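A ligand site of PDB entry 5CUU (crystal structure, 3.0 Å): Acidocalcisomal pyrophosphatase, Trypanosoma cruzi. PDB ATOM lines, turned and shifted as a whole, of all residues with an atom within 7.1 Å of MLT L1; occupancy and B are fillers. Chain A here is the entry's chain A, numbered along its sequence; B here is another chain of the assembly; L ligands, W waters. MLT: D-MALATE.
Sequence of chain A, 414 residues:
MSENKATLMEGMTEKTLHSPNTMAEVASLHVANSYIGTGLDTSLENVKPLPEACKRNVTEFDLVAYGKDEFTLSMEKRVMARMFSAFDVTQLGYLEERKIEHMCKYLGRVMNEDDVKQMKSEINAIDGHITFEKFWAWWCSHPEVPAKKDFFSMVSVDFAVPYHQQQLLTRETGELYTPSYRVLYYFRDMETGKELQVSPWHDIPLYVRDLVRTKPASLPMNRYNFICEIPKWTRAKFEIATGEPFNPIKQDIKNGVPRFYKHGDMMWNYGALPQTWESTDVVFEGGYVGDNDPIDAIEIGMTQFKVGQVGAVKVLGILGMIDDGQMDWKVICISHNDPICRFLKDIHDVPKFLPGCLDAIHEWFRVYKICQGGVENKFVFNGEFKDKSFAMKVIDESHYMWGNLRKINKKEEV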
ATOM      1  N   VAL A 208     -34.567  -4.773  -4.986  1.00  0.00           N
ATOM      2  CA  VAL A 208     -34.682  -3.348  -5.115  1.00  0.00           C
ATOM      3  C   VAL A 208     -33.411  -2.862  -5.768  1.00  0.00           C
ATOM      4  O   VAL A 208     -32.396  -2.713  -5.120  1.00  0.00           O
ATOM      5  CB  VAL A 208     -34.868  -2.647  -3.788  1.00  0.00           C
ATOM      6  CG1 VAL A 208     -34.703  -1.130  -3.978  1.00  0.00           C
ATOM      7  CG2 VAL A 208     -36.241  -2.938  -3.262  1.00  0.00           C
ATOM      8  N   ARG A 209     -33.463  -2.616  -7.066  1.00  0.00           N
ATOM      9  CA  ARG A 209     -32.261  -2.162  -7.715  1.00  0.00           C
ATOM     10  C   ARG A 209     -32.323  -0.704  -8.140  1.00  0.00           C
ATOM     11  O   ARG A 209     -33.409  -0.166  -8.320  1.00  0.00           O
ATOM     12  CB  ARG A 209     -31.951  -3.078  -8.907  1.00  0.00           C
ATOM     13  CG  ARG A 209     -31.302  -4.419  -8.489  1.00  0.00           C
ATOM     14  CD  ARG A 209     -31.154  -5.381  -9.682  1.00  0.00           C
ATOM     15  NE  ARG A 209     -30.638  -6.690  -9.278  1.00  0.00           N
ATOM     16  CZ  ARG A 209     -30.895  -7.840  -9.905  1.00  0.00           C
ATOM     17  NH1 ARG A 209     -31.689  -7.865 -10.984  1.00  0.00           N
ATOM     18  NH2 ARG A 209     -30.364  -8.972  -9.440  1.00  0.00           N
ATOM     19  N   ASP A 210     -31.138  -0.095  -8.244  1.00  0.00           N
ATOM     20  CA  ASP A 210     -30.966   1.309  -8.657  1.00  0.00           C
ATOM     21  C   ASP A 210     -30.481   1.430 -10.082  1.00  0.00           C
ATOM     22  O   ASP A 210     -29.543   0.731 -10.463  1.00  0.00           O
ATOM     23  CB  ASP A 210     -29.956   2.007  -7.760  1.00  0.00           C
ATOM     24  CG  ASP A 210     -30.509   2.281  -6.406  1.00  0.00           C
ATOM     25  OD1 ASP A 210     -31.618   2.887  -6.376  1.00  0.00           O
ATOM     26  OD2 ASP A 210     -29.848   1.878  -5.395  1.00  0.00           O
ATOM     27  N   ARG A 213     -26.125   2.592  -9.398  1.00  0.00           N
ATOM     28  CA  ARG A 213     -25.804   2.266  -8.010  1.00  0.00           C
ATOM     29  C   ARG A 213     -24.641   3.120  -7.608  1.00  0.00           C
ATOM     30  O   ARG A 213     -23.593   3.101  -8.258  1.00  0.00           O
ATOM     31  CB  ARG A 213     -25.421   0.780  -7.884  1.00  0.00           C
ATOM     32  CG  ARG A 213     -25.214   0.260  -6.419  1.00  0.00           C
ATOM     33  CD  ARG A 213     -26.144  -0.953  -6.026  1.00  0.00           C
ATOM     34  NE  ARG A 213     -25.961  -1.361  -4.639  1.00  0.00           N
ATOM     35  CZ  ARG A 213     -24.765  -1.691  -4.141  1.00  0.00           C
ATOM     36  NH1 ARG A 213     -23.690  -1.686  -4.929  1.00  0.00           N
ATOM     37  NH2 ARG A 213     -24.641  -1.962  -2.851  1.00  0.00           N
ATOM     38  N   LYS A 215     -23.698   3.258  -4.185  1.00  0.00           N
ATOM     39  CA  LYS A 215     -23.085   2.653  -3.004  1.00  0.00           C
ATOM     40  C   LYS A 215     -21.828   1.972  -3.495  1.00  0.00           C
ATOM     41  O   LYS A 215     -21.830   1.361  -4.560  1.00  0.00           O
ATOM     42  CB  LYS A 215     -23.985   1.596  -2.408  1.00  0.00           C
ATOM     43  CG  LYS A 215     -25.318   2.093  -2.009  1.00  0.00           C
ATOM     44  CD  LYS A 215     -26.126   0.998  -1.341  1.00  0.00           C
ATOM     45  CE  LYS A 215     -27.356   1.592  -0.653  1.00  0.00           C
ATOM     46  NZ  LYS A 215     -27.051   2.118   0.732  1.00  0.00           N
ATOM     47  N   LEU A 219     -19.215  -2.965  -1.423  1.00  0.00           N
ATOM     48  CA  LEU A 219     -20.387  -3.333  -0.644  1.00  0.00           C
ATOM     49  C   LEU A 219     -21.345  -4.078  -1.544  1.00  0.00           C
ATOM     50  O   LEU A 219     -21.881  -3.509  -2.469  1.00  0.00           O
ATOM     51  CB  LEU A 219     -21.055  -2.070  -0.127  1.00  0.00           C
ATOM     52  CG  LEU A 219     -22.300  -2.179   0.738  1.00  0.00           C
ATOM     53  CD1 LEU A 219     -21.911  -2.195   2.206  1.00  0.00           C
ATOM     54  CD2 LEU A 219     -23.201  -0.992   0.444  1.00  0.00           C
ATOM     55  N   PRO A 220     -21.563  -5.387  -1.307  1.00  0.00           N
ATOM     56  CA  PRO A 220     -22.470  -6.199  -2.127  1.00  0.00           C
ATOM     57  C   PRO A 220     -23.932  -5.756  -1.988  1.00  0.00           C
ATOM     58  O   PRO A 220     -24.298  -5.114  -1.015  1.00  0.00           O
ATOM     59  CB  PRO A 220     -22.239  -7.609  -1.610  1.00  0.00           C
ATOM     60  CG  PRO A 220     -20.843  -7.574  -1.230  1.00  0.00           C
ATOM     61  CD  PRO A 220     -20.739  -6.273  -0.474  1.00  0.00           C
ATOM     62  N   MET A 221     -24.754  -6.149  -2.955  1.00  0.00           N
ATOM     63  CA  MET A 221     -26.156  -5.765  -2.951  1.00  0.00           C
ATOM     64  C   MET A 221     -27.086  -6.516  -2.026  1.00  0.00           C
ATOM     65  O   MET A 221     -27.269  -7.734  -2.138  1.00  0.00           O
ATOM     66  CB  MET A 221     -26.712  -5.819  -4.367  1.00  0.00           C
ATOM     67  CG  MET A 221     -25.940  -4.984  -5.358  1.00  0.00           C
ATOM     68  SD  MET A 221     -26.726  -5.025  -7.006  1.00  0.00           S
ATOM     69  CE  MET A 221     -28.618  -4.332  -6.545  1.00  0.00           C
ATOM     70  N   ASN A 222     -27.701  -5.774  -1.107  1.00  0.00           N
ATOM     71  CA  ASN A 222     -28.613  -6.372  -0.150  1.00  0.00           C
ATOM     72  C   ASN A 222     -29.838  -5.538   0.127  1.00  0.00           C
ATOM     73  O   ASN A 222     -29.967  -4.951   1.173  1.00  0.00           O
ATOM     74  CB  ASN A 222     -27.876  -6.665   1.153  1.00  0.00           C
ATOM     75  CG  ASN A 222     -28.471  -7.840   1.879  1.00  0.00           C
ATOM     76  OD1 ASN A 222     -29.499  -8.332   1.451  1.00  0.00           O
ATOM     77  ND2 ASN A 222     -27.852  -8.296   2.963  1.00  0.00           N
ATOM     78  N   ARG A 223     -30.770  -5.501  -0.806  1.00  0.00           N
ATOM     79  CA  ARG A 223     -31.991  -4.760  -0.621  1.00  0.00           C
ATOM     80  C   ARG A 223     -33.100  -5.517  -1.387  1.00  0.00           C
ATOM     81  O   ARG A 223     -33.134  -5.478  -2.635  1.00  0.00           O
ATOM     82  CB  ARG A 223     -31.796  -3.324  -1.153  1.00  0.00           C
ATOM     83  CG  ARG A 223     -32.766  -2.267  -0.580  1.00  0.00           C
ATOM     84  CD  ARG A 223     -32.353  -0.863  -1.008  1.00  0.00           C
ATOM     85  NE  ARG A 223     -32.864   0.208  -0.139  1.00  0.00           N
ATOM     86  CZ  ARG A 223     -32.144   0.849   0.808  1.00  0.00           C
ATOM     87  NH1 ARG A 223     -30.857   0.533   1.017  1.00  0.00           N
ATOM     88  NH2 ARG A 223     -32.720   1.826   1.544  1.00  0.00           N
ATOM     89  N   VAL A 313     -35.894  -4.501   2.811  1.00  0.00           N
ATOM     90  CA  VAL A 313     -35.237  -5.155   3.889  1.00  0.00           C
ATOM     91  C   VAL A 313     -33.840  -5.608   3.455  1.00  0.00           C
ATOM     92  O   VAL A 313     -33.504  -5.609   2.278  1.00  0.00           O
ATOM     93  CB  VAL A 313     -36.086  -6.389   4.384  1.00  0.00           C
ATOM     94  CG1 VAL A 313     -37.533  -5.985   4.707  1.00  0.00           C
ATOM     95  CG2 VAL A 313     -36.052  -7.502   3.334  1.00  0.00           C
ATOM     96  N   LYS A 314     -33.052  -5.961   4.463  1.00  0.00           N
ATOM     97  CA  LYS A 314     -31.690  -6.472   4.345  1.00  0.00           C
ATOM     98  C   LYS A 314     -31.792  -7.951   4.817  1.00  0.00           C
ATOM     99  O   LYS A 314     -32.268  -8.251   5.913  1.00  0.00           O
ATOM    100  CB  LYS A 314     -30.759  -5.684   5.276  1.00  0.00           C
ATOM    101  CG  LYS A 314     -29.315  -5.726   4.865  1.00  0.00           C
ATOM    102  CD  LYS A 314     -28.339  -5.485   5.997  1.00  0.00           C
ATOM    103  CE  LYS A 314     -28.434  -4.078   6.507  1.00  0.00           C
ATOM    104  NZ  LYS A 314     -27.082  -3.658   6.926  1.00  0.00           N
ATOM    105  N   HIS A 336     -34.748  -1.775   6.142  1.00  0.00           N
ATOM    106  CA  HIS A 336     -33.646  -0.846   5.936  1.00  0.00           C
ATOM    107  C   HIS A 336     -33.761   0.478   6.711  1.00  0.00           C
ATOM    108  O   HIS A 336     -32.815   1.260   6.797  1.00  0.00           O
ATOM    109  CB  HIS A 336     -33.514  -0.548   4.454  1.00  0.00           C
ATOM    110  CG  HIS A 336     -32.609  -1.502   3.728  1.00  0.00           C
ATOM    111  ND1 HIS A 336     -31.245  -1.504   3.883  1.00  0.00           N
ATOM    112  CD2 HIS A 336     -32.882  -2.472   2.821  1.00  0.00           C
ATOM    113  CE1 HIS A 336     -30.707  -2.430   3.106  1.00  0.00           C
ATOM    114  NE2 HIS A 336     -31.685  -3.032   2.448  1.00  0.00           N
ATOM    115  N   CYS A 341     -30.442  -1.368  11.604  1.00  0.00           N
ATOM    116  CA  CYS A 341     -30.181  -2.097  10.391  1.00  0.00           C
ATOM    117  C   CYS A 341     -28.711  -2.004   9.962  1.00  0.00           C
ATOM    118  O   CYS A 341     -28.097  -3.012   9.701  1.00  0.00           O
ATOM    119  CB  CYS A 341     -31.113  -1.614   9.279  1.00  0.00           C
ATOM    120  SG  CYS A 341     -30.350  -1.531   7.635  1.00  0.00           S
ATOM    121  N   LEU A 344     -26.047  -4.249  11.406  1.00  0.00           N
ATOM    122  CA  LEU A 344     -26.281  -5.690  11.303  1.00  0.00           C
ATOM    123  C   LEU A 344     -25.820  -6.142   9.941  1.00  0.00           C
ATOM    124  O   LEU A 344     -26.475  -5.910   8.916  1.00  0.00           O
ATOM    125  CB  LEU A 344     -27.769  -6.043  11.477  1.00  0.00           C
ATOM    126  CG  LEU A 344     -28.520  -5.760  12.757  1.00  0.00           C
ATOM    127  CD1 LEU A 344     -29.628  -6.785  12.933  1.00  0.00           C
ATOM    128  CD2 LEU A 344     -27.546  -5.795  13.918  1.00  0.00           C
ATOM    129  N   GLN B 165     -28.818  -2.229 -14.574  1.00  0.00           N
ATOM    130  CA  GLN B 165     -28.361  -1.473 -13.428  1.00  0.00           C
ATOM    131  C   GLN B 165     -26.872  -1.267 -13.648  1.00  0.00           C
ATOM    132  O   GLN B 165     -26.177  -2.191 -14.052  1.00  0.00           O
ATOM    133  CB  GLN B 165     -28.649  -2.249 -12.149  1.00  0.00           C
ATOM    134  CG  GLN B 165     -27.934  -1.720 -10.946  1.00  0.00           C
ATOM    135  CD  GLN B 165     -28.419  -2.369  -9.691  1.00  0.00           C
ATOM    136  OE1 GLN B 165     -28.566  -3.604  -9.624  1.00  0.00           O
ATOM    137  NE2 GLN B 165     -28.694  -1.553  -8.678  1.00  0.00           N
ATOM    138  N   MET B 190     -23.768  -4.188 -14.668  1.00  0.00           N
ATOM    139  CA  MET B 190     -23.901  -5.297 -13.712  1.00  0.00           C
ATOM    140  C   MET B 190     -24.521  -6.535 -14.348  1.00  0.00           C
ATOM    141  O   MET B 190     -25.023  -7.397 -13.617  1.00  0.00           O
ATOM    142  CB  MET B 190     -24.723  -4.863 -12.519  1.00  0.00           C
ATOM    143  CG  MET B 190     -24.047  -3.874 -11.693  1.00  0.00           C
ATOM    144  SD  MET B 190     -25.092  -3.387 -10.299  1.00  0.00           S
ATOM    145  CE  MET B 190     -24.099  -4.079  -8.810  1.00  0.00           C
HETATM  146  C1  MLT L   1     -27.642  -2.205  -1.949  1.00  0.00           C
HETATM  147  O1  MLT L   1     -27.960  -1.213  -2.613  1.00  0.00           O
HETATM  148  O2  MLT L   1     -27.089  -3.111  -2.527  1.00  0.00           O
HETATM  149  C2  MLT L   1     -27.929  -2.289  -0.425  1.00  0.00           C
HETATM  150  O3  MLT L   1     -28.600  -1.134   0.074  1.00  0.00           O
HETATM  151  C3  MLT L   1     -26.610  -2.499   0.358  1.00  0.00           C
HETATM  152  C4  MLT L   1     -26.835  -2.559   1.870  1.00  0.00           C
HETATM  153  O4  MLT L   1     -27.918  -2.432   2.321  1.00  0.00           O
HETATM  154  O5  MLT L   1     -25.817  -2.749   2.705  1.00  0.00           O
HETATM  155  C1  MLT L   2     -29.781   1.983   4.063  1.00  0.00           C
HETATM  156  O1  MLT L   2     -28.731   2.070   3.412  1.00  0.00           O
HETATM  157  O2  MLT L   2     -29.863   1.174   4.990  1.00  0.00           O
HETATM  158  C2  MLT L   2     -30.996   2.853   3.715  1.00  0.00           C
HETATM  159  O3  MLT L   2     -30.739   3.734   2.602  1.00  0.00           O
HETATM  160  C3  MLT L   2     -31.446   3.638   4.981  1.00  0.00           C
HETATM  161  C4  MLT L   2     -32.640   4.513   4.681  1.00  0.00           C
HETATM  162  O4  MLT L   2     -33.127   4.533   3.561  1.00  0.00           O
HETATM  163  O5  MLT L   2     -33.187   5.252   5.671  1.00  0.00           O
HETATM  164  O   HOH W   1     -25.768  -0.557   5.277  1.00  0.00           O
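An oxygen (O2) of MLT L1 lies within salt-bridge range of the guanidinium group (NH2) of Arg 213.
NH1 of Arg 223 sits at hydrogen-bond distance from O3 of MLT L1 (3.0 Å).
N of Asn 222 sits at hydrogen-bond distance from O2 of MLT L1 (3.1 Å).
A ring nitrogen (ND1) of His 336 sits at hydrogen-bond distance from an oxygen (O2) of MLT L2 (3.2 Å).
The guanidinium group (NH2) of Arg 223 is in salt-bridge range of an oxygen (O4) of MLT L2.
An oxygen (O1) of MLT L2 is in salt-bridge range of the side-chain amino group (NZ) of Lys 215, 3.2 Å away.
The guanidinium group (NH2) of Arg 213 lies within hydrogen-bond range of the backbone carbonyl oxygen (O) of Leu 219, at 3.2 Å.
The side-chain sulfur (SD) of Met 221 lies close to the side-chain amide oxygen (OE1) of Gln 165 of chain B (3.5 Å).
The backbone carbonyl oxygen (O) of Asn 222 sits at hydrogen-bond distance from a ring nitrogen (NE2) of His 336, 2.9 Å away.
NE2 of His 336 sits at hydrogen-bond distance from O of Val 313 (3.2 Å).
The backbone NH of Val 208 lies within hydrogen-bond range of the backbone carbonyl oxygen of Arg 223 (2.8 Å).
Merely in contact with MLT L1: Met 221, His 336, Lys 215, Leu 219 and Pro 220.
Eight residues have an atom within 4 Å of MLT L1: Arg 213, Lys 215, Leu 219, Pro 220, Met 221, Asn 222, Arg 223 and His 336.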
